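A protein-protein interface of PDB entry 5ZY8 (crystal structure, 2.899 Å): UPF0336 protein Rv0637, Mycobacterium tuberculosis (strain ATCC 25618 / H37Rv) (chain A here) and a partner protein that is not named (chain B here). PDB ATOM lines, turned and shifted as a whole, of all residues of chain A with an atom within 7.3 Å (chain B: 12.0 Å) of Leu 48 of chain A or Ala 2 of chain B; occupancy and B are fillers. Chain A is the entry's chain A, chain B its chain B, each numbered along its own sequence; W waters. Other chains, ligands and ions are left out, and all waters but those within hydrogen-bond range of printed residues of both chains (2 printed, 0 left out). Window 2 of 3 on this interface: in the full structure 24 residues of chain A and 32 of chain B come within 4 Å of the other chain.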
ATOM      1  N   HIS A  36      -0.900  19.203 -20.186  1.00  0.00           N
ATOM      2  CA  HIS A  36      -0.451  17.825 -20.364  1.00  0.00           C
ATOM      3  C   HIS A  36      -0.465  17.490 -21.850  1.00  0.00           C
ATOM      4  O   HIS A  36      -1.488  17.697 -22.517  1.00  0.00           O
ATOM      5  CB  HIS A  36      -1.342  16.855 -19.599  1.00  0.00           C
ATOM      6  CG  HIS A  36      -0.732  15.500 -19.410  1.00  0.00           C
ATOM      7  ND1 HIS A  36      -0.447  14.661 -20.462  1.00  0.00           N
ATOM      8  CD2 HIS A  36      -0.393  14.824 -18.286  1.00  0.00           C
ATOM      9  CE1 HIS A  36       0.061  13.536 -19.996  1.00  0.00           C
ATOM     10  NE2 HIS A  36       0.103  13.607 -18.679  1.00  0.00           N
ATOM     11  N   PRO A  37       0.630  16.967 -22.406  1.00  0.00           N
ATOM     12  CA  PRO A  37       0.681  16.766 -23.865  1.00  0.00           C
ATOM     13  C   PRO A  37      -0.320  15.752 -24.391  1.00  0.00           C
ATOM     14  O   PRO A  37      -0.634  15.787 -25.592  1.00  0.00           O
ATOM     15  CB  PRO A  37       2.125  16.301 -24.101  1.00  0.00           C
ATOM     16  CG  PRO A  37       2.591  15.794 -22.786  1.00  0.00           C
ATOM     17  CD  PRO A  37       1.919  16.653 -21.766  1.00  0.00           C
ATOM     18  N   ALA A  38      -0.878  14.894 -23.531  1.00  0.00           N
ATOM     19  CA  ALA A  38      -1.861  13.941 -24.016  1.00  0.00           C
ATOM     20  C   ALA A  38      -3.175  14.614 -24.387  1.00  0.00           C
ATOM     21  O   ALA A  38      -4.005  13.982 -25.052  1.00  0.00           O
ATOM     22  CB  ALA A  38      -2.091  12.838 -22.991  1.00  0.00           C
ATOM     23  N   GLU A  42      -1.185  12.945 -30.099  1.00  0.00           N
ATOM     24  CA  GLU A  42      -1.515  11.522 -30.084  1.00  0.00           C
ATOM     25  C   GLU A  42      -0.317  10.671 -29.692  1.00  0.00           C
ATOM     26  O   GLU A  42      -0.495   9.570 -29.163  1.00  0.00           O
ATOM     27  CB  GLU A  42      -2.066  11.073 -31.436  1.00  0.00           C
ATOM     28  CG  GLU A  42      -1.890  12.082 -32.550  1.00  0.00           C
ATOM     29  CD  GLU A  42      -3.063  13.064 -32.692  1.00  0.00           C
ATOM     30  OE1 GLU A  42      -4.251  12.690 -32.541  1.00  0.00           O
ATOM     31  OE2 GLU A  42      -2.777  14.244 -32.969  1.00  0.00           O
ATOM     32  N   GLU A  43       0.895  11.170 -29.915  1.00  0.00           N
ATOM     33  CA  GLU A  43       2.085  10.462 -29.459  1.00  0.00           C
ATOM     34  C   GLU A  43       2.122  10.394 -27.939  1.00  0.00           C
ATOM     35  O   GLU A  43       2.403   9.338 -27.355  1.00  0.00           O
ATOM     36  CB  GLU A  43       3.326  11.156 -29.997  1.00  0.00           C
ATOM     37  CG  GLU A  43       3.227  11.371 -31.484  1.00  0.00           C
ATOM     38  CD  GLU A  43       4.440  10.890 -32.245  1.00  0.00           C
ATOM     39  OE1 GLU A  43       4.352  10.867 -33.494  1.00  0.00           O
ATOM     40  OE2 GLU A  43       5.479  10.578 -31.609  1.00  0.00           O
ATOM     41  N   ALA A  44       1.862  11.530 -27.282  1.00  0.00           N
ATOM     42  CA  ALA A  44       1.813  11.567 -25.824  1.00  0.00           C
ATOM     43  C   ALA A  44       0.717  10.654 -25.286  1.00  0.00           C
ATOM     44  O   ALA A  44       0.902   9.983 -24.264  1.00  0.00           O
ATOM     45  CB  ALA A  44       1.603  13.006 -25.346  1.00  0.00           C
ATOM     46  N   ALA A  45      -0.442  10.643 -25.947  1.00  0.00           N
ATOM     47  CA  ALA A  45      -1.514   9.734 -25.554  1.00  0.00           C
ATOM     48  C   ALA A  45      -1.116   8.272 -25.759  1.00  0.00           C
ATOM     49  O   ALA A  45      -1.513   7.393 -24.980  1.00  0.00           O
ATOM     50  CB  ALA A  45      -2.790  10.069 -26.329  1.00  0.00           C
ATOM     51  N   ALA A  46      -0.340   7.990 -26.806  1.00  0.00           N
ATOM     52  CA  ALA A  46       0.130   6.625 -27.008  1.00  0.00           C
ATOM     53  C   ALA A  46       0.992   6.151 -25.835  1.00  0.00           C
ATOM     54  O   ALA A  46       0.919   4.980 -25.441  1.00  0.00           O
ATOM     55  CB  ALA A  46       0.895   6.523 -28.331  1.00  0.00           C
ATOM     56  N   ASP A  47       1.803   7.043 -25.255  1.00  0.00           N
ATOM     57  CA  ASP A  47       2.609   6.644 -24.100  1.00  0.00           C
ATOM     58  C   ASP A  47       1.747   6.185 -22.930  1.00  0.00           C
ATOM     59  O   ASP A  47       2.211   5.414 -22.081  1.00  0.00           O
ATOM     60  CB  ASP A  47       3.501   7.789 -23.631  1.00  0.00           C
ATOM     61  CG  ASP A  47       4.651   8.048 -24.561  1.00  0.00           C
ATOM     62  OD1 ASP A  47       5.173   7.070 -25.148  1.00  0.00           O
ATOM     63  OD2 ASP A  47       5.037   9.236 -24.689  1.00  0.00           O
ATOM     64  N   LEU A  48       0.519   6.677 -22.838  1.00  0.00           N
ATOM     65  CA  LEU A  48      -0.371   6.307 -21.754  1.00  0.00           C
ATOM     66  C   LEU A  48      -1.351   5.196 -22.123  1.00  0.00           C
ATOM     67  O   LEU A  48      -2.179   4.820 -21.283  1.00  0.00           O
ATOM     68  CB  LEU A  48      -1.124   7.550 -21.283  1.00  0.00           C
ATOM     69  CG  LEU A  48      -0.258   8.708 -20.779  1.00  0.00           C
ATOM     70  CD1 LEU A  48      -1.140   9.843 -20.331  1.00  0.00           C
ATOM     71  CD2 LEU A  48       0.640   8.259 -19.633  1.00  0.00           C
ATOM     72  N   GLY A  49      -1.275   4.650 -23.341  1.00  0.00           N
ATOM     73  CA  GLY A  49      -2.110   3.532 -23.738  1.00  0.00           C
ATOM     74  C   GLY A  49      -3.276   3.846 -24.665  1.00  0.00           C
ATOM     75  O   GLY A  49      -3.954   2.910 -25.109  1.00  0.00           O
ATOM     76  N   TYR A  50      -3.509   5.111 -25.004  1.00  0.00           N
ATOM     77  CA  TYR A  50      -4.682   5.517 -25.776  1.00  0.00           C
ATOM     78  C   TYR A  50      -4.316   5.717 -27.247  1.00  0.00           C
ATOM     79  O   TYR A  50      -3.183   6.090 -27.567  1.00  0.00           O
ATOM     80  CB  TYR A  50      -5.317   6.794 -25.183  1.00  0.00           C
ATOM     81  CG  TYR A  50      -5.354   6.796 -23.659  1.00  0.00           C
ATOM     82  CD1 TYR A  50      -4.439   7.514 -22.907  1.00  0.00           C
ATOM     83  CD2 TYR A  50      -6.290   6.029 -22.977  1.00  0.00           C
ATOM     84  CE1 TYR A  50      -4.476   7.494 -21.500  1.00  0.00           C
ATOM     85  CE2 TYR A  50      -6.336   5.996 -21.570  1.00  0.00           C
ATOM     86  CZ  TYR A  50      -5.421   6.719 -20.836  1.00  0.00           C
ATOM     87  OH  TYR A  50      -5.445   6.680 -19.445  1.00  0.00           O
ATOM     88  N   ASP A  51      -5.256   5.388 -28.140  1.00  0.00           N
ATOM     89  CA  ASP A  51      -5.027   5.473 -29.578  1.00  0.00           C
ATOM     90  C   ASP A  51      -5.510   6.782 -30.200  1.00  0.00           C
ATOM     91  O   ASP A  51      -5.390   6.954 -31.422  1.00  0.00           O
ATOM     92  CB  ASP A  51      -5.693   4.286 -30.289  1.00  0.00           C
ATOM     93  CG  ASP A  51      -5.028   3.958 -31.629  1.00  0.00           C
ATOM     94  OD1 ASP A  51      -3.793   4.182 -31.757  1.00  0.00           O
ATOM     95  OD2 ASP A  51      -5.730   3.473 -32.550  1.00  0.00           O
ATOM     96  N   VAL A  54      -6.659  12.516 -25.467  1.00  0.00           N
ATOM     97  CA  VAL A  54      -7.670  12.546 -24.410  1.00  0.00           C
ATOM     98  C   VAL A  54      -8.353  13.904 -24.354  1.00  0.00           C
ATOM     99  O   VAL A  54      -7.698  14.951 -24.433  1.00  0.00           O
ATOM    100  CB  VAL A  54      -7.027  12.199 -23.061  1.00  0.00           C
ATOM    101  CG1 VAL A  54      -8.102  12.096 -21.977  1.00  0.00           C
ATOM    102  CG2 VAL A  54      -6.222  10.909 -23.178  1.00  0.00           C
ATOM    103  N   ALA B   2       3.850  10.736 -17.561  1.00  0.00           N
ATOM    104  CA  ALA B   2       3.530   9.344 -17.213  1.00  0.00           C
ATOM    105  C   ALA B   2       2.686   9.219 -15.940  1.00  0.00           C
ATOM    106  O   ALA B   2       2.666  10.120 -15.104  1.00  0.00           O
ATOM    107  CB  ALA B   2       4.799   8.552 -17.046  1.00  0.00           C
ATOM    108  N   LEU B   3       1.994   8.086 -15.808  1.00  0.00           N
ATOM    109  CA  LEU B   3       1.048   7.874 -14.714  1.00  0.00           C
ATOM    110  C   LEU B   3       1.774   7.683 -13.377  1.00  0.00           C
ATOM    111  O   LEU B   3       2.638   6.809 -13.247  1.00  0.00           O
ATOM    112  CB  LEU B   3       0.141   6.681 -15.014  1.00  0.00           C
ATOM    113  CG  LEU B   3      -0.881   6.300 -13.927  1.00  0.00           C
ATOM    114  CD1 LEU B   3      -1.799   7.476 -13.603  1.00  0.00           C
ATOM    115  CD2 LEU B   3      -1.709   5.086 -14.317  1.00  0.00           C
ATOM    116  N   ARG B   4       1.427   8.513 -12.394  1.00  0.00           N
ATOM    117  CA  ARG B   4       2.012   8.437 -11.056  1.00  0.00           C
ATOM    118  C   ARG B   4       1.844   7.039 -10.447  1.00  0.00           C
ATOM    119  O   ARG B   4       0.788   6.409 -10.581  1.00  0.00           O
ATOM    120  CB  ARG B   4       1.382   9.486 -10.145  1.00  0.00           C
ATOM    121  CG  ARG B   4       2.030   9.549  -8.793  1.00  0.00           C
ATOM    122  CD  ARG B   4       1.515  10.720  -7.997  1.00  0.00           C
ATOM    123  NE  ARG B   4       1.816  11.988  -8.645  1.00  0.00           N
ATOM    124  CZ  ARG B   4       2.948  12.654  -8.489  1.00  0.00           C
ATOM    125  NH1 ARG B   4       3.874  12.190  -7.668  1.00  0.00           N
ATOM    126  NH2 ARG B   4       3.135  13.794  -9.128  1.00  0.00           N
ATOM    127  N   GLU B   5       2.913   6.531  -9.818  1.00  0.00           N
ATOM    128  CA  GLU B   5       2.860   5.218  -9.173  1.00  0.00           C
ATOM    129  C   GLU B   5       2.013   5.269  -7.907  1.00  0.00           C
ATOM    130  O   GLU B   5       2.242   6.118  -7.039  1.00  0.00           O
ATOM    131  CB  GLU B   5       4.279   4.784  -8.785  1.00  0.00           C
ATOM    132  CG  GLU B   5       5.212   4.377  -9.915  1.00  0.00           C
ATOM    133  CD  GLU B   5       5.059   2.923 -10.297  1.00  0.00           C
ATOM    134  OE1 GLU B   5       4.295   2.202  -9.613  1.00  0.00           O
ATOM    135  OE2 GLU B   5       5.701   2.497 -11.284  1.00  0.00           O
ATOM    136  N   PHE B   6       1.091   4.301  -7.758  1.00  0.00           N
ATOM    137  CA  PHE B   6       0.251   4.246  -6.556  1.00  0.00           C
ATOM    138  C   PHE B   6       1.084   4.140  -5.285  1.00  0.00           C
ATOM    139  O   PHE B   6       0.764   4.763  -4.267  1.00  0.00           O
ATOM    140  CB  PHE B   6      -0.715   3.065  -6.625  1.00  0.00           C
ATOM    141  CG  PHE B   6      -1.607   2.944  -5.418  1.00  0.00           C
ATOM    142  CD1 PHE B   6      -2.713   3.776  -5.274  1.00  0.00           C
ATOM    143  CD2 PHE B   6      -1.317   2.040  -4.407  1.00  0.00           C
ATOM    144  CE1 PHE B   6      -3.539   3.683  -4.161  1.00  0.00           C
ATOM    145  CE2 PHE B   6      -2.137   1.937  -3.281  1.00  0.00           C
ATOM    146  CZ  PHE B   6      -3.248   2.759  -3.157  1.00  0.00           C
ATOM    147  N   SER B   7       2.147   3.337  -5.328  1.00  0.00           N
ATOM    148  CA  SER B   7       2.961   3.067  -4.152  1.00  0.00           C
ATOM    149  C   SER B   7       3.726   4.296  -3.672  1.00  0.00           C
ATOM    150  O   SER B   7       4.224   4.291  -2.541  1.00  0.00           O
ATOM    151  CB  SER B   7       3.925   1.912  -4.434  1.00  0.00           C
ATOM    152  OG  SER B   7       4.873   2.257  -5.428  1.00  0.00           O
ATOM    153  N   SER B   8       3.836   5.335  -4.496  1.00  0.00           N
ATOM    154  CA  SER B   8       4.558   6.533  -4.105  1.00  0.00           C
ATOM    155  C   SER B   8       3.692   7.553  -3.376  1.00  0.00           C
ATOM    156  O   SER B   8       4.239   8.550  -2.879  1.00  0.00           O
ATOM    157  CB  SER B   8       5.164   7.216  -5.326  1.00  0.00           C
ATOM    158  OG  SER B   8       4.147   7.837  -6.089  1.00  0.00           O
ATOM    159  N   VAL B   9       2.388   7.318  -3.247  1.00  0.00           N
ATOM    160  CA  VAL B   9       1.477   8.327  -2.738  1.00  0.00           C
ATOM    161  C   VAL B   9       1.118   7.905  -1.326  1.00  0.00           C
ATOM    162  O   VAL B   9       0.798   6.736  -1.073  1.00  0.00           O
ATOM    163  CB  VAL B   9       0.232   8.460  -3.635  1.00  0.00           C
ATOM    164  CG1 VAL B   9      -0.801   9.392  -3.009  1.00  0.00           C
ATOM    165  CG2 VAL B   9       0.639   8.940  -5.014  1.00  0.00           C
ATOM    166  N   GLY B  67      -9.331  20.807 -13.749  1.00  0.00           N
ATOM    167  CA  GLY B  67      -9.101  19.508 -14.360  1.00  0.00           C
ATOM    168  C   GLY B  67      -7.681  19.408 -14.872  1.00  0.00           C
ATOM    169  O   GLY B  67      -7.025  18.374 -14.722  1.00  0.00           O
ATOM    170  N   GLY B  68      -7.181  20.497 -15.462  1.00  0.00           N
ATOM    171  CA  GLY B  68      -5.804  20.528 -15.926  1.00  0.00           C
ATOM    172  C   GLY B  68      -4.871  20.395 -14.738  1.00  0.00           C
ATOM    173  O   GLY B  68      -3.854  19.698 -14.794  1.00  0.00           O
ATOM    174  N   TYR B  69      -5.197  21.110 -13.659  1.00  0.00           N
ATOM    175  CA  TYR B  69      -4.422  21.085 -12.426  1.00  0.00           C
ATOM    176  C   TYR B  69      -4.300  19.630 -11.993  1.00  0.00           C
ATOM    177  O   TYR B  69      -3.208  19.125 -11.712  1.00  0.00           O
ATOM    178  CB  TYR B  69      -5.071  21.956 -11.344  1.00  0.00           C
ATOM    179  CG  TYR B  69      -4.384  21.879  -9.987  1.00  0.00           C
ATOM    180  CD1 TYR B  69      -3.164  22.521  -9.788  1.00  0.00           C
ATOM    181  CD2 TYR B  69      -4.925  21.166  -8.922  1.00  0.00           C
ATOM    182  CE1 TYR B  69      -2.503  22.477  -8.571  1.00  0.00           C
ATOM    183  CE2 TYR B  69      -4.263  21.110  -7.685  1.00  0.00           C
ATOM    184  CZ  TYR B  69      -3.051  21.769  -7.518  1.00  0.00           C
ATOM    185  OH  TYR B  69      -2.389  21.722  -6.305  1.00  0.00           O
ATOM    186  N   VAL B  70      -5.435  18.939 -11.936  1.00  0.00           N
ATOM    187  CA  VAL B  70      -5.458  17.605 -11.368  1.00  0.00           C
ATOM    188  C   VAL B  70      -4.749  16.658 -12.315  1.00  0.00           C
ATOM    189  O   VAL B  70      -4.023  15.756 -11.877  1.00  0.00           O
ATOM    190  CB  VAL B  70      -6.924  17.168 -11.158  1.00  0.00           C
ATOM    191  CG1 VAL B  70      -7.060  15.668 -11.234  1.00  0.00           C
ATOM    192  CG2 VAL B  70      -7.431  17.642  -9.829  1.00  0.00           C
ATOM    193  N   THR B  71      -4.856  16.905 -13.620  1.00  0.00           N
ATOM    194  CA  THR B  71      -4.248  15.985 -14.559  1.00  0.00           C
ATOM    195  C   THR B  71      -2.731  16.057 -14.521  1.00  0.00           C
ATOM    196  O   THR B  71      -2.065  15.022 -14.645  1.00  0.00           O
ATOM    197  CB  THR B  71      -4.703  16.344 -15.970  1.00  0.00           C
ATOM    198  OG1 THR B  71      -6.128  16.281 -16.063  1.00  0.00           O
ATOM    199  CG2 THR B  71      -4.059  15.440 -17.006  1.00  0.00           C
ATOM    200  N   SER B  72      -2.163  17.235 -14.253  1.00  0.00           N
ATOM    201  CA  SER B  72      -0.706  17.317 -14.184  1.00  0.00           C
ATOM    202  C   SER B  72      -0.131  16.515 -13.029  1.00  0.00           C
ATOM    203  O   SER B  72       0.951  15.934 -13.159  1.00  0.00           O
ATOM    204  CB  SER B  72      -0.264  18.774 -14.089  1.00  0.00           C
ATOM    205  OG  SER B  72      -0.333  19.384 -15.369  1.00  0.00           O
ATOM    206  N   TRP B  73      -0.823  16.481 -11.884  1.00  0.00           N
ATOM    207  CA  TRP B  73      -0.342  15.664 -10.773  1.00  0.00           C
ATOM    208  C   TRP B  73      -0.503  14.164 -11.029  1.00  0.00           C
ATOM    209  O   TRP B  73       0.420  13.382 -10.760  1.00  0.00           O
ATOM    210  CB  TRP B  73      -1.022  16.083  -9.468  1.00  0.00           C
ATOM    211  CG  TRP B  73      -0.477  15.295  -8.339  1.00  0.00           C
ATOM    212  CD1 TRP B  73       0.665  15.552  -7.639  1.00  0.00           C
ATOM    213  CD2 TRP B  73      -1.056  14.129  -7.748  1.00  0.00           C
ATOM    214  NE1 TRP B  73       0.853  14.598  -6.674  1.00  0.00           N
ATOM    215  CE2 TRP B  73      -0.192  13.714  -6.716  1.00  0.00           C
ATOM    216  CE3 TRP B  73      -2.216  13.393  -7.996  1.00  0.00           C
ATOM    217  CZ2 TRP B  73      -0.455  12.595  -5.924  1.00  0.00           C
ATOM    218  CZ3 TRP B  73      -2.476  12.278  -7.211  1.00  0.00           C
ATOM    219  CH2 TRP B  73      -1.598  11.891  -6.185  1.00  0.00           C
ATOM    220  N   VAL B  74      -1.663  13.748 -11.547  1.00  0.00           N
ATOM    221  CA  VAL B  74      -1.915  12.334 -11.835  1.00  0.00           C
ATOM    222  C   VAL B  74      -0.933  11.809 -12.876  1.00  0.00           C
ATOM    223  O   VAL B  74      -0.406  10.693 -12.758  1.00  0.00           O
ATOM    224  CB  VAL B  74      -3.378  12.126 -12.267  1.00  0.00           C
ATOM    225  CG1 VAL B  74      -3.598  10.711 -12.730  1.00  0.00           C
ATOM    226  CG2 VAL B  74      -4.293  12.432 -11.109  1.00  0.00           C
ATOM    227  N   GLY B  75      -0.731  12.572 -13.945  1.00  0.00           N
ATOM    228  CA  GLY B  75       0.208  12.198 -14.977  1.00  0.00           C
ATOM    229  C   GLY B  75      -0.449  11.563 -16.175  1.00  0.00           C
ATOM    230  O   GLY B  75       0.253  11.213 -17.129  1.00  0.00           O
ATOM    231  N   ASP B  76      -1.783  11.482 -16.174  1.00  0.00           N
ATOM    232  CA  ASP B  76      -2.623  10.886 -17.190  1.00  0.00           C
ATOM    233  C   ASP B  76      -4.077  11.298 -16.980  1.00  0.00           C
ATOM    234  O   ASP B  76      -4.738  10.821 -16.049  1.00  0.00           O
ATOM    235  CB  ASP B  76      -2.495   9.363 -17.070  1.00  0.00           C
ATOM    236  CG  ASP B  76      -3.380   8.602 -18.057  1.00  0.00           C
ATOM    237  OD1 ASP B  76      -3.416   7.342 -17.979  1.00  0.00           O
ATOM    238  OD2 ASP B  76      -4.049   9.250 -18.897  1.00  0.00           O
ATOM    239  N   PRO B  77      -4.619  12.136 -17.868  1.00  0.00           N
ATOM    240  CA  PRO B  77      -6.031  12.524 -17.753  1.00  0.00           C
ATOM    241  C   PRO B  77      -6.968  11.336 -17.807  1.00  0.00           C
ATOM    242  O   PRO B  77      -8.008  11.331 -17.135  1.00  0.00           O
ATOM    243  CB  PRO B  77      -6.233  13.478 -18.936  1.00  0.00           C
ATOM    244  CG  PRO B  77      -5.152  13.126 -19.898  1.00  0.00           C
ATOM    245  CD  PRO B  77      -3.991  12.645 -19.102  1.00  0.00           C
ATOM    246  N   GLY B  78      -6.583  10.304 -18.569  1.00  0.00           N
ATOM    247  CA  GLY B  78      -7.353   9.083 -18.762  1.00  0.00           C
ATOM    248  C   GLY B  78      -7.510   8.252 -17.516  1.00  0.00           C
ATOM    249  O   GLY B  78      -8.417   7.416 -17.452  1.00  0.00           O
ATOM    250  N   ALA B  79      -6.708   8.531 -16.495  1.00  0.00           N
ATOM    251  CA  ALA B  79      -6.706   7.792 -15.245  1.00  0.00           C
ATOM    252  C   ALA B  79      -7.742   8.344 -14.274  1.00  0.00           C
ATOM    253  O   ALA B  79      -8.053   7.685 -13.275  1.00  0.00           O
ATOM    254  CB  ALA B  79      -5.308   7.809 -14.607  1.00  0.00           C
ATOM    255  N   VAL B  80      -8.271   9.539 -14.528  1.00  0.00           N
ATOM    256  CA  VAL B  80      -9.175  10.172 -13.579  1.00  0.00           C
ATOM    257  C   VAL B  80     -10.541   9.501 -13.696  1.00  0.00           C
ATOM    258  O   VAL B  80     -11.060   9.307 -14.804  1.00  0.00           O
ATOM    259  CB  VAL B  80      -9.261  11.688 -13.840  1.00  0.00           C
ATOM    260  CG1 VAL B  80     -10.236  12.368 -12.877  1.00  0.00           C
ATOM    261  CG2 VAL B  80      -7.876  12.329 -13.704  1.00  0.00           C
ATOM    262  N   VAL B 118      -6.725   6.863  -5.708  1.00  0.00           N
ATOM    263  CA  VAL B 118      -6.485   7.928  -4.734  1.00  0.00           C
ATOM    264  C   VAL B 118      -7.564   8.991  -4.927  1.00  0.00           C
ATOM    265  O   VAL B 118      -8.096   9.168  -6.027  1.00  0.00           O
ATOM    266  CB  VAL B 118      -5.081   8.572  -4.828  1.00  0.00           C
ATOM    267  CG1 VAL B 118      -3.994   7.502  -4.786  1.00  0.00           C
ATOM    268  CG2 VAL B 118      -4.949   9.490  -6.019  1.00  0.00           C
ATOM    269  N   ALA B 139      -8.595   9.132  -9.073  1.00  0.00           N
ATOM    270  CA  ALA B 139      -7.907   8.553 -10.213  1.00  0.00           C
ATOM    271  C   ALA B 139      -7.380   7.193  -9.797  1.00  0.00           C
ATOM    272  O   ALA B 139      -7.103   6.955  -8.617  1.00  0.00           O
ATOM    273  CB  ALA B 139      -6.762   9.442 -10.708  1.00  0.00           C
ATOM    274  N   LYS B 140      -7.221   6.316 -10.789  1.00  0.00           N
ATOM    275  CA  LYS B 140      -6.608   5.007 -10.603  1.00  0.00           C
ATOM    276  C   LYS B 140      -5.148   5.103 -11.032  1.00  0.00           C
ATOM    277  O   LYS B 140      -4.861   5.445 -12.186  1.00  0.00           O
ATOM    278  CB  LYS B 140      -7.368   3.928 -11.379  1.00  0.00           C
ATOM    279  CG  LYS B 140      -6.761   2.531 -11.296  1.00  0.00           C
ATOM    280  CD  LYS B 140      -7.585   1.516 -12.101  1.00  0.00           C
ATOM    281  CE  LYS B 140      -6.992   0.098 -12.072  1.00  0.00           C
ATOM    282  NZ  LYS B 140      -7.208  -0.625 -10.786  1.00  0.00           N
ATOM    283  N   LEU B 141      -4.233   4.887 -10.089  1.00  0.00           N
ATOM    284  CA  LEU B 141      -2.814   5.075 -10.351  1.00  0.00           C
ATOM    285  C   LEU B 141      -2.185   3.749 -10.777  1.00  0.00           C
ATOM    286  O   LEU B 141      -2.810   2.688 -10.701  1.00  0.00           O
ATOM    287  CB  LEU B 141      -2.105   5.652  -9.126  1.00  0.00           C
ATOM    288  CG  LEU B 141      -2.601   7.037  -8.693  1.00  0.00           C
ATOM    289  CD1 LEU B 141      -1.642   7.668  -7.696  1.00  0.00           C
ATOM    290  CD2 LEU B 141      -2.798   7.935  -9.904  1.00  0.00           C
ATOM    291  N   ALA B 142      -0.911   3.810 -11.166  1.00  0.00           N
ATOM    292  CA  ALA B 142      -0.228   2.650 -11.764  1.00  0.00           C
ATOM    293  C   ALA B 142       0.297   1.623 -10.757  1.00  0.00           C
ATOM    294  O   ALA B 142       0.921   1.969  -9.758  1.00  0.00           O
ATOM    295  CB  ALA B 142       0.921   3.134 -12.640  1.00  0.00           C
HETATM  296  O   HOH W   1      -1.145   5.176 -18.575  1.00  0.00           O
HETATM  297  O   HOH W   2      -6.714   4.637 -18.400  1.00  0.00           O
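The side-chain hydroxyl of Tyr 50 of chain A is in hydrogen-bond range of the side-chain carboxylate of Asp 76 of chain B, at 2.6 Å.
The backbone carbonyl oxygen (O) of Gly 75 of chain B lies within hydrogen-bond range of a ring nitrogen (NE2) of His 36 of chain A (2.9 Å).
O of Gly 67 of chain B lies within hydrogen-bond range of OG1 of Thr 71 of chain B (2.6 Å).
The backbone NH of Lys 140 of chain B lies within hydrogen-bond range of the backbone carbonyl oxygen of Ala 79 of chain B, at 3.0 Å.
O of Ala 45 of chain A lies within hydrogen-bond range of N of Tyr 50 of chain A (3.0 Å).
The backbone NH (N) of Gly 78 of chain B sits at hydrogen-bond distance from the side-chain carboxylate (OD2) of Asp 76 of chain B (2.8 Å).
O of Ala 38 of chain A lies within hydrogen-bond range of N of Val 54 of chain A, 3.1 Å away.
ND1 of His 36 of chain A sits at hydrogen-bond distance from N of Ala 38 of chain A (3.1 Å).
Thr 71 of chain B touches His 36 of chain A.
Asp 76 of chain B touches His 36 of chain A (N to NE2, 3.8 Å).
CD2 of Leu 48 of chain A touches CA of Ala 2 of chain B, 3.9 Å away.
Leu 48 of chain A touches Gly 75 of chain B.
Leu 48 of chain A touches Asp 76 of chain B (CD1 to OD2, 3.3 Å).
Tyr 50 of chain A touches Gly 78 of chain B.
N of Ala 79 of chain B touches OH of Tyr 50 of chain A (3.7 Å).
CG of Pro 77 of chain B touches CG1 of Val 54 of chain A (3.8 Å).
Leu 48 of chain A touches just these residues of chain B: Ala 2 (3.9 Å), Gly 75 (3.8 Å) and Asp 76 (3.3 Å).
Ala 2 of chain B touches just one residue of chain A: Leu 48.
Ala 38 of chain A touches none of the printed residues of chain B.
No residue of chain B comes within 4 Å of Ala 44 of chain A.
Ala 45 of chain A touches none of the printed residues of chain B.
No residue of chain B comes within 4 Å of Ala 46 of chain A.
No residue of chain B comes within 4 Å of Asp 47 of chain A.
No residue of chain B comes within 4 Å of Gly 49 of chain A.
Tyr 50 of chain A touches just these residues of chain B: Asp 76, Gly 78 and Ala 79.
Of the printed residues of chain A, Gly 75 of chain B touches His 36 and Leu 48.
Of the printed residues of chain A, Pro 77 of chain B touches Val 54.
Of the printed residues of chain B, Val 54 of chain A touches Pro 77.
Of the printed residues of chain A, Asp 76 of chain B touches His 36, Leu 48 and Tyr 50.
Of the printed residues of chain A, Gly 78 of chain B touches Tyr 50.
The nearest residue of chain A that does not touch Ala 2 of chain B is His 36 of chain A (4.9 Å).
The nearest printed residue of chain A that does not touch Asp 76 of chain B is Val 54 of chain A (5.1 Å).
Of the 14 printed residues of chain A, 4 touch a printed residue of chain B.
Hydrophobic or aromatic side chains of chain A that line the printed part of chain B: His 36, Leu 48, Tyr 50 and Val 54.
Along chain A the printed residues that touch a printed residue of chain B span positions 36 to 54.
Hydrophobic or aromatic side chains of chain B that line the printed part of chain A: Pro 77.
Among the printed residues, 10 pairs touch across the chains.
Among the printed residues, no Asp or Glu carboxylate lies within 4 Å of a Lys or Arg side-chain nitrogen of the other chain.
Water W2 bridges the side-chain hydroxyl (OH) of Tyr 50 of chain A (2.6 Å) and the backbone carbonyl oxygen (O) of Gly 78 of chain B (3.4 Å).
Water W1 lies within hydrogen-bond range of O of Leu 48 of chain A and OD1 of Asp 76 of chain B.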
